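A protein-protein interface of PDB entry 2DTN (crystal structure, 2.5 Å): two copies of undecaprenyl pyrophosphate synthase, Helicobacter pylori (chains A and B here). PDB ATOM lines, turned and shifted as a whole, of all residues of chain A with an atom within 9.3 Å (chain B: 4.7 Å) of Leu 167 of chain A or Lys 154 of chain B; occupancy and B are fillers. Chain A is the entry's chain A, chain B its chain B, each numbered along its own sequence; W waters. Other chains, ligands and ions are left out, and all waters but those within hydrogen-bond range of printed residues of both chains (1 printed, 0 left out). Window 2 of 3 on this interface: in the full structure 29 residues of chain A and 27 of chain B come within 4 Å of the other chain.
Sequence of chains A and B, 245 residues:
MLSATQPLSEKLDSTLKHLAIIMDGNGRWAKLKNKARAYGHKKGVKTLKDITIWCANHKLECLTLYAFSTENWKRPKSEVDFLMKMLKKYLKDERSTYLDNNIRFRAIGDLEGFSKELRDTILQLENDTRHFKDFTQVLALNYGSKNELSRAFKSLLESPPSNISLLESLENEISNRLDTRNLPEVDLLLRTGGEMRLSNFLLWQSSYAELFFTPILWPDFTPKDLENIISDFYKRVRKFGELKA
OE2 of Glu 168 of chain A lies within salt-bridge range of NZ of Lys 154 of chain B (3.0 Å). The backbone NH (N) of Leu 170 of chain A lies within hydrogen-bond range of the side-chain hydroxyl (OG) of Ser 150 of chain B.
Phe 153 of chain B touches Phe 153 of chain A. CZ of Phe 153 of chain A touches CB of Leu 156 of chain B, at 3.4 Å. Leu 157 of chain B touches Leu 156 of chain A. Leu 167 of chain A touches Lys 154 of chain B (O to NZ, 3.5 Å). Ser 150 of chain B touches Ser 169 of chain A (OG to C, 3.6 Å). Phe 153 of chain B touches Leu 170 of chain A. Leu 170 of chain A touches Lys 154 of chain B. Glu 171 of chain A touches Ser 150 of chain B. CD1 of Ile 174 of chain A touches CD2 of Phe 153 of chain B (3.4 Å).
Of chain B, only Lys 154 (3.5 Å) comes within 4 Å of Leu 167 of chain A. Lys 154 of chain B touches three residues of chain A. No residue of chain A comes within 4 Å of Ser 155 of chain B. Of the printed residues of chain B, Ile 174 of chain A touches Phe 153. Of the printed residues of chain B, Phe 153 of chain A touches Phe 153 (3.7 Å) and Leu 156 (3.4 Å). Of the printed residues of chain A, Phe 153 of chain B touches Phe 153, Leu 170 and Ile 174. Of the printed residues of chain B, Glu 168 of chain A touches Lys 154. Of the printed residues of chain B, Ser 169 of chain A touches Ser 150 (3.6 Å). Ser 162 of chain A touches none of the printed residues of chain B. Arg 177 of chain A touches none of the printed residues of chain B. The nearest printed residue of chain B that does not touch Leu 167 of chain A is Ser 150 of chain B (7.9 Å). The nearest residue of chain A that does not touch Lys 154 of chain B is Ile 164 of chain A (5.2 Å).
Of the 9 printed residues of chain B, 5 touch a printed residue of chain A. Among the printed residues, Asp or Glu carboxylates within 4 Å of a Lys or Arg side-chain nitrogen of the other chain: Glu 168 of chain A with Lys 154 of chain B (3.0 Å).
Phe 153 of chain A touches its own counterpart, Phe 153 of chain B. Phe 153 of chain A touches Leu 156 of chain B, but with the chains exchanged Leu 156 of chain A does not touch Phe 153 of chain B (4.3 Å). Of the 11 pairs that touch across the chains among the printed residues, 1 has its exchanged pair printed and touching as well.
Water W1 bridges NZ of Lys 154 of chain B (2.5 Å) and OE2 of Glu 168 of chain A (2.8 Å).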
ATOM      1  N   PHE A 153      35.479 -32.992  -8.918  1.00  0.00           N
ATOM      2  CA  PHE A 153      34.948 -31.633  -8.980  1.00  0.00           C
ATOM      3  C   PHE A 153      36.091 -30.640  -9.050  1.00  0.00           C
ATOM      4  O   PHE A 153      36.079 -29.711  -9.856  1.00  0.00           O
ATOM      5  CB  PHE A 153      34.121 -31.295  -7.739  1.00  0.00           C
ATOM      6  CG  PHE A 153      33.748 -29.843  -7.649  1.00  0.00           C
ATOM      7  CD1 PHE A 153      32.729 -29.323  -8.438  1.00  0.00           C
ATOM      8  CD2 PHE A 153      34.455 -28.982  -6.817  1.00  0.00           C
ATOM      9  CE1 PHE A 153      32.416 -27.956  -8.402  1.00  0.00           C
ATOM     10  CE2 PHE A 153      34.157 -27.621  -6.772  1.00  0.00           C
ATOM     11  CZ  PHE A 153      33.134 -27.104  -7.567  1.00  0.00           C
ATOM     12  N   LEU A 156      37.369 -30.145 -12.412  1.00  0.00           N
ATOM     13  CA  LEU A 156      36.584 -29.327 -13.341  1.00  0.00           C
ATOM     14  C   LEU A 156      36.699 -27.836 -13.035  1.00  0.00           C
ATOM     15  O   LEU A 156      36.496 -26.997 -13.904  1.00  0.00           O
ATOM     16  CB  LEU A 156      35.108 -29.739 -13.300  1.00  0.00           C
ATOM     17  CG  LEU A 156      34.771 -31.126 -13.853  1.00  0.00           C
ATOM     18  CD1 LEU A 156      33.367 -31.519 -13.434  1.00  0.00           C
ATOM     19  CD2 LEU A 156      34.908 -31.121 -15.370  1.00  0.00           C
ATOM     20  N   PRO A 160      38.335 -26.775 -16.507  1.00  0.00           N
ATOM     21  CA  PRO A 160      37.000 -26.975 -17.066  1.00  0.00           C
ATOM     22  C   PRO A 160      37.098 -27.337 -18.540  1.00  0.00           C
ATOM     23  O   PRO A 160      38.137 -27.123 -19.165  1.00  0.00           O
ATOM     24  CB  PRO A 160      36.324 -25.628 -16.832  1.00  0.00           C
ATOM     25  CG  PRO A 160      37.461 -24.667 -16.929  1.00  0.00           C
ATOM     26  CD  PRO A 160      38.551 -25.363 -16.150  1.00  0.00           C
ATOM     27  N   PRO A 161      36.029 -27.922 -19.107  1.00  0.00           N
ATOM     28  CA  PRO A 161      36.030 -28.299 -20.525  1.00  0.00           C
ATOM     29  C   PRO A 161      35.659 -27.084 -21.374  1.00  0.00           C
ATOM     30  O   PRO A 161      34.693 -26.389 -21.077  1.00  0.00           O
ATOM     31  CB  PRO A 161      34.980 -29.398 -20.582  1.00  0.00           C
ATOM     32  CG  PRO A 161      33.985 -28.927 -19.596  1.00  0.00           C
ATOM     33  CD  PRO A 161      34.831 -28.451 -18.433  1.00  0.00           C
ATOM     34  N   SER A 162      36.436 -26.828 -22.422  1.00  0.00           N
ATOM     35  CA  SER A 162      36.198 -25.681 -23.297  1.00  0.00           C
ATOM     36  C   SER A 162      34.718 -25.330 -23.508  1.00  0.00           C
ATOM     37  O   SER A 162      34.322 -24.173 -23.297  1.00  0.00           O
ATOM     38  CB  SER A 162      36.882 -25.913 -24.647  1.00  0.00           C
ATOM     39  OG  SER A 162      38.293 -25.892 -24.504  1.00  0.00           O
ATOM     40  N   ASN A 163      33.898 -26.312 -23.903  1.00  0.00           N
ATOM     41  CA  ASN A 163      32.465 -26.037 -24.145  1.00  0.00           C
ATOM     42  C   ASN A 163      31.642 -26.133 -22.854  1.00  0.00           C
ATOM     43  O   ASN A 163      30.444 -26.445 -22.893  1.00  0.00           O
ATOM     44  CB  ASN A 163      31.907 -27.023 -25.190  1.00  0.00           C
ATOM     45  CG  ASN A 163      31.930 -28.465 -24.694  1.00  0.00           C
ATOM     46  OD1 ASN A 163      32.210 -28.726 -23.506  1.00  0.00           O
ATOM     47  ND2 ASN A 163      31.634 -29.415 -25.592  1.00  0.00           N
ATOM     48  N   ILE A 164      32.284 -25.861 -21.717  1.00  0.00           N
ATOM     49  CA  ILE A 164      31.630 -25.922 -20.412  1.00  0.00           C
ATOM     50  C   ILE A 164      30.528 -24.876 -20.267  1.00  0.00           C
ATOM     51  O   ILE A 164      29.573 -25.056 -19.508  1.00  0.00           O
ATOM     52  CB  ILE A 164      32.665 -25.728 -19.272  1.00  0.00           C
ATOM     53  CG1 ILE A 164      31.975 -25.847 -17.906  1.00  0.00           C
ATOM     54  CG2 ILE A 164      33.354 -24.364 -19.420  1.00  0.00           C
ATOM     55  CD1 ILE A 164      31.246 -27.151 -17.689  1.00  0.00           C
ATOM     56  N   SER A 165      30.677 -23.785 -21.007  1.00  0.00           N
ATOM     57  CA  SER A 165      29.714 -22.694 -20.971  1.00  0.00           C
ATOM     58  C   SER A 165      28.457 -23.080 -21.745  1.00  0.00           C
ATOM     59  O   SER A 165      27.366 -22.586 -21.465  1.00  0.00           O
ATOM     60  CB  SER A 165      30.352 -21.433 -21.570  1.00  0.00           C
ATOM     61  OG  SER A 165      29.502 -20.312 -21.460  1.00  0.00           O
ATOM     62  N   LEU A 166      28.621 -23.976 -22.713  1.00  0.00           N
ATOM     63  CA  LEU A 166      27.513 -24.437 -23.544  1.00  0.00           C
ATOM     64  C   LEU A 166      26.869 -25.689 -22.954  1.00  0.00           C
ATOM     65  O   LEU A 166      25.911 -26.225 -23.511  1.00  0.00           O
ATOM     66  CB  LEU A 166      28.015 -24.745 -24.958  1.00  0.00           C
ATOM     67  CG  LEU A 166      28.781 -23.635 -25.681  1.00  0.00           C
ATOM     68  CD1 LEU A 166      29.321 -24.163 -26.997  1.00  0.00           C
ATOM     69  CD2 LEU A 166      27.866 -22.444 -25.913  1.00  0.00           C
ATOM     70  N   LEU A 167      27.401 -26.148 -21.824  1.00  0.00           N
ATOM     71  CA  LEU A 167      26.900 -27.348 -21.162  1.00  0.00           C
ATOM     72  C   LEU A 167      25.848 -27.079 -20.095  1.00  0.00           C
ATOM     73  O   LEU A 167      25.802 -25.999 -19.499  1.00  0.00           O
ATOM     74  CB  LEU A 167      28.066 -28.124 -20.545  1.00  0.00           C
ATOM     75  CG  LEU A 167      29.007 -28.781 -21.555  1.00  0.00           C
ATOM     76  CD1 LEU A 167      30.254 -29.278 -20.839  1.00  0.00           C
ATOM     77  CD2 LEU A 167      28.283 -29.924 -22.262  1.00  0.00           C
ATOM     78  N   GLU A 168      25.001 -28.078 -19.867  1.00  0.00           N
ATOM     79  CA  GLU A 168      23.943 -27.990 -18.871  1.00  0.00           C
ATOM     80  C   GLU A 168      24.059 -29.217 -17.973  1.00  0.00           C
ATOM     81  O   GLU A 168      23.862 -29.135 -16.761  1.00  0.00           O
ATOM     82  CB  GLU A 168      22.573 -27.967 -19.553  1.00  0.00           C
ATOM     83  CG  GLU A 168      21.490 -27.280 -18.737  1.00  0.00           C
ATOM     84  CD  GLU A 168      21.731 -25.785 -18.593  1.00  0.00           C
ATOM     85  OE1 GLU A 168      21.774 -25.080 -19.625  1.00  0.00           O
ATOM     86  OE2 GLU A 168      21.878 -25.311 -17.447  1.00  0.00           O
ATOM     87  N   SER A 169      24.380 -30.355 -18.584  1.00  0.00           N
ATOM     88  CA  SER A 169      24.554 -31.605 -17.856  1.00  0.00           C
ATOM     89  C   SER A 169      26.046 -31.951 -17.808  1.00  0.00           C
ATOM     90  O   SER A 169      26.737 -31.949 -18.835  1.00  0.00           O
ATOM     91  CB  SER A 169      23.772 -32.728 -18.540  1.00  0.00           C
ATOM     92  OG  SER A 169      23.940 -33.962 -17.860  1.00  0.00           O
ATOM     93  N   LEU A 170      26.540 -32.254 -16.612  1.00  0.00           N
ATOM     94  CA  LEU A 170      27.948 -32.576 -16.432  1.00  0.00           C
ATOM     95  C   LEU A 170      28.227 -34.054 -16.144  1.00  0.00           C
ATOM     96  O   LEU A 170      29.370 -34.428 -15.909  1.00  0.00           O
ATOM     97  CB  LEU A 170      28.519 -31.715 -15.303  1.00  0.00           C
ATOM     98  CG  LEU A 170      28.467 -30.197 -15.505  1.00  0.00           C
ATOM     99  CD1 LEU A 170      28.814 -29.492 -14.206  1.00  0.00           C
ATOM    100  CD2 LEU A 170      29.426 -29.786 -16.609  1.00  0.00           C
ATOM    101  N   GLU A 171      27.192 -34.889 -16.181  1.00  0.00           N
ATOM    102  CA  GLU A 171      27.351 -36.316 -15.911  1.00  0.00           C
ATOM    103  C   GLU A 171      28.477 -36.935 -16.722  1.00  0.00           C
ATOM    104  O   GLU A 171      29.308 -37.675 -16.195  1.00  0.00           O
ATOM    105  CB  GLU A 171      26.055 -37.069 -16.210  1.00  0.00           C
ATOM    106  CG  GLU A 171      24.813 -36.463 -15.575  1.00  0.00           C
ATOM    107  CD  GLU A 171      23.584 -37.339 -15.747  1.00  0.00           C
ATOM    108  OE1 GLU A 171      22.460 -36.794 -15.725  1.00  0.00           O
ATOM    109  OE2 GLU A 171      23.743 -38.569 -15.901  1.00  0.00           O
ATOM    110  N   ASN A 172      28.495 -36.641 -18.018  1.00  0.00           N
ATOM    111  CA  ASN A 172      29.536 -37.181 -18.902  1.00  0.00           C
ATOM    112  C   ASN A 172      30.890 -36.539 -18.591  1.00  0.00           C
ATOM    113  O   ASN A 172      31.937 -37.181 -18.742  1.00  0.00           O
ATOM    114  CB  ASN A 172      29.168 -36.944 -20.379  1.00  0.00           C
ATOM    115  CG  ASN A 172      30.304 -37.301 -21.317  1.00  0.00           C
ATOM    116  OD1 ASN A 172      31.325 -36.585 -21.363  1.00  0.00           O
ATOM    117  ND2 ASN A 172      30.162 -38.423 -22.056  1.00  0.00           N
ATOM    118  N   GLU A 173      30.864 -35.284 -18.155  1.00  0.00           N
ATOM    119  CA  GLU A 173      32.090 -34.574 -17.800  1.00  0.00           C
ATOM    120  C   GLU A 173      32.658 -35.188 -16.527  1.00  0.00           C
ATOM    121  O   GLU A 173      33.846 -35.450 -16.420  1.00  0.00           O
ATOM    122  CB  GLU A 173      31.805 -33.092 -17.534  1.00  0.00           C
ATOM    123  CG  GLU A 173      31.239 -32.299 -18.710  1.00  0.00           C
ATOM    124  CD  GLU A 173      32.194 -32.227 -19.876  1.00  0.00           C
ATOM    125  OE1 GLU A 173      33.388 -31.947 -19.649  1.00  0.00           O
ATOM    126  OE2 GLU A 173      31.754 -32.442 -21.023  1.00  0.00           O
ATOM    127  N   ILE A 174      31.783 -35.396 -15.554  1.00  0.00           N
ATOM    128  CA  ILE A 174      32.163 -35.967 -14.270  1.00  0.00           C
ATOM    129  C   ILE A 174      32.686 -37.393 -14.395  1.00  0.00           C
ATOM    130  O   ILE A 174      33.711 -37.747 -13.818  1.00  0.00           O
ATOM    131  CB  ILE A 174      30.961 -35.980 -13.317  1.00  0.00           C
ATOM    132  CG1 ILE A 174      30.582 -34.543 -12.935  1.00  0.00           C
ATOM    133  CG2 ILE A 174      31.276 -36.819 -12.107  1.00  0.00           C
ATOM    134  CD1 ILE A 174      29.203 -34.395 -12.273  1.00  0.00           C
ATOM    135  N   ARG A 177      36.302 -37.638 -15.187  1.00  0.00           N
ATOM    136  CA  ARG A 177      37.275 -36.993 -14.310  1.00  0.00           C
ATOM    137  C   ARG A 177      37.469 -37.897 -13.091  1.00  0.00           C
ATOM    138  O   ARG A 177      38.347 -37.665 -12.259  1.00  0.00           O
ATOM    139  CB  ARG A 177      36.794 -35.604 -13.868  1.00  0.00           C
ATOM    140  CG  ARG A 177      36.646 -34.590 -15.004  1.00  0.00           C
ATOM    141  CD  ARG A 177      37.898 -34.518 -15.853  1.00  0.00           C
ATOM    142  NE  ARG A 177      37.799 -33.526 -16.924  1.00  0.00           N
ATOM    143  CZ  ARG A 177      37.884 -32.211 -16.745  1.00  0.00           C
ATOM    144  NH1 ARG A 177      38.071 -31.708 -15.531  1.00  0.00           N
ATOM    145  NH2 ARG A 177      37.789 -31.396 -17.786  1.00  0.00           N
ATOM    146  N   SER B 150      25.126 -33.495 -10.815  1.00  0.00           N
ATOM    147  CA  SER B 150      25.490 -32.671 -11.951  1.00  0.00           C
ATOM    148  C   SER B 150      24.988 -31.246 -11.788  1.00  0.00           C
ATOM    149  O   SER B 150      25.638 -30.305 -12.220  1.00  0.00           O
ATOM    150  CB  SER B 150      24.929 -33.274 -13.241  1.00  0.00           C
ATOM    151  OG  SER B 150      25.177 -32.420 -14.348  1.00  0.00           O
ATOM    152  N   ARG B 151      23.831 -31.083 -11.164  1.00  0.00           N
ATOM    153  CA  ARG B 151      23.282 -29.747 -10.974  1.00  0.00           C
ATOM    154  C   ARG B 151      23.975 -29.010  -9.840  1.00  0.00           C
ATOM    155  O   ARG B 151      24.094 -27.783  -9.869  1.00  0.00           O
ATOM    156  CB  ARG B 151      21.773 -29.814 -10.718  1.00  0.00           C
ATOM    157  CG  ARG B 151      20.960 -30.157 -11.955  1.00  0.00           C
ATOM    158  CD  ARG B 151      19.454 -30.037 -11.719  1.00  0.00           C
ATOM    159  NE  ARG B 151      18.900 -31.202 -11.035  1.00  0.00           N
ATOM    160  CZ  ARG B 151      18.570 -31.243  -9.746  1.00  0.00           C
ATOM    161  NH1 ARG B 151      18.732 -30.169  -8.981  1.00  0.00           N
ATOM    162  NH2 ARG B 151      18.081 -32.367  -9.224  1.00  0.00           N
ATOM    163  N   ALA B 152      24.436 -29.752  -8.842  1.00  0.00           N
ATOM    164  CA  ALA B 152      25.123 -29.141  -7.712  1.00  0.00           C
ATOM    165  C   ALA B 152      26.533 -28.729  -8.142  1.00  0.00           C
ATOM    166  O   ALA B 152      27.066 -27.723  -7.688  1.00  0.00           O
ATOM    167  CB  ALA B 152      25.188 -30.122  -6.541  1.00  0.00           C
ATOM    168  N   PHE B 153      27.137 -29.518  -9.021  1.00  0.00           N
ATOM    169  CA  PHE B 153      28.476 -29.209  -9.497  1.00  0.00           C
ATOM    170  C   PHE B 153      28.427 -27.930 -10.299  1.00  0.00           C
ATOM    171  O   PHE B 153      29.215 -27.014 -10.077  1.00  0.00           O
ATOM    172  CB  PHE B 153      29.005 -30.350 -10.363  1.00  0.00           C
ATOM    173  CG  PHE B 153      29.701 -31.427  -9.580  1.00  0.00           C
ATOM    174  CD1 PHE B 153      29.343 -31.691  -8.267  1.00  0.00           C
ATOM    175  CD2 PHE B 153      30.691 -32.207 -10.169  1.00  0.00           C
ATOM    176  CE1 PHE B 153      29.960 -32.720  -7.560  1.00  0.00           C
ATOM    177  CE2 PHE B 153      31.310 -33.237  -9.461  1.00  0.00           C
ATOM    178  CZ  PHE B 153      30.942 -33.493  -8.160  1.00  0.00           C
ATOM    179  N   LYS B 154      27.484 -27.891 -11.231  1.00  0.00           N
ATOM    180  CA  LYS B 154      27.262 -26.751 -12.103  1.00  0.00           C
ATOM    181  C   LYS B 154      27.004 -25.506 -11.261  1.00  0.00           C
ATOM    182  O   LYS B 154      27.435 -24.406 -11.599  1.00  0.00           O
ATOM    183  CB  LYS B 154      26.054 -27.038 -12.992  1.00  0.00           C
ATOM    184  CG  LYS B 154      25.588 -25.871 -13.825  1.00  0.00           C
ATOM    185  CD  LYS B 154      26.600 -25.501 -14.890  1.00  0.00           C
ATOM    186  CE  LYS B 154      25.992 -24.482 -15.830  1.00  0.00           C
ATOM    187  NZ  LYS B 154      24.666 -24.981 -16.320  1.00  0.00           N
ATOM    188  N   SER B 155      26.295 -25.693 -10.156  1.00  0.00           N
ATOM    189  CA  SER B 155      25.982 -24.601  -9.265  1.00  0.00           C
ATOM    190  C   SER B 155      27.255 -24.077  -8.617  1.00  0.00           C
ATOM    191  O   SER B 155      27.455 -22.869  -8.509  1.00  0.00           O
ATOM    192  CB  SER B 155      25.013 -25.077  -8.189  1.00  0.00           C
ATOM    193  OG  SER B 155      24.686 -24.021  -7.309  1.00  0.00           O
ATOM    194  N   LEU B 156      28.111 -24.997  -8.187  1.00  0.00           N
ATOM    195  CA  LEU B 156      29.365 -24.645  -7.536  1.00  0.00           C
ATOM    196  C   LEU B 156      30.289 -23.892  -8.473  1.00  0.00           C
ATOM    197  O   LEU B 156      30.822 -22.844  -8.110  1.00  0.00           O
ATOM    198  CB  LEU B 156      30.053 -25.902  -7.016  1.00  0.00           C
ATOM    199  CG  LEU B 156      29.299 -26.513  -5.838  1.00  0.00           C
ATOM    200  CD1 LEU B 156      29.881 -27.861  -5.468  1.00  0.00           C
ATOM    201  CD2 LEU B 156      29.375 -25.551  -4.669  1.00  0.00           C
ATOM    202  N   LEU B 157      30.483 -24.428  -9.673  1.00  0.00           N
ATOM    203  CA  LEU B 157      31.323 -23.771 -10.662  1.00  0.00           C
ATOM    204  C   LEU B 157      30.782 -22.362 -10.842  1.00  0.00           C
ATOM    205  O   LEU B 157      31.446 -21.381 -10.520  1.00  0.00           O
ATOM    206  CB  LEU B 157      31.260 -24.525 -11.984  1.00  0.00           C
ATOM    207  CG  LEU B 157      31.955 -25.884 -11.968  1.00  0.00           C
ATOM    208  CD1 LEU B 157      31.663 -26.628 -13.262  1.00  0.00           C
ATOM    209  CD2 LEU B 157      33.453 -25.684 -11.769  1.00  0.00           C
ATOM    210  N   GLU B 158      29.558 -22.285 -11.348  1.00  0.00           N
ATOM    211  CA  GLU B 158      28.866 -21.020 -11.567  1.00  0.00           C
ATOM    212  C   GLU B 158      29.058 -20.051 -10.397  1.00  0.00           C
ATOM    213  O   GLU B 158      29.568 -18.942 -10.577  1.00  0.00           O
ATOM    214  CB  GLU B 158      27.371 -21.294 -11.772  1.00  0.00           C
ATOM    215  CG  GLU B 158      26.460 -20.111 -11.470  1.00  0.00           C
ATOM    216  CD  GLU B 158      25.000 -20.519 -11.317  1.00  0.00           C
ATOM    217  OE1 GLU B 158      24.400 -20.969 -12.320  1.00  0.00           O
ATOM    218  OE2 GLU B 158      24.456 -20.396 -10.192  1.00  0.00           O
HETATM  219  O   HOH W   1      22.758 -23.761 -15.242  1.00  0.00           O
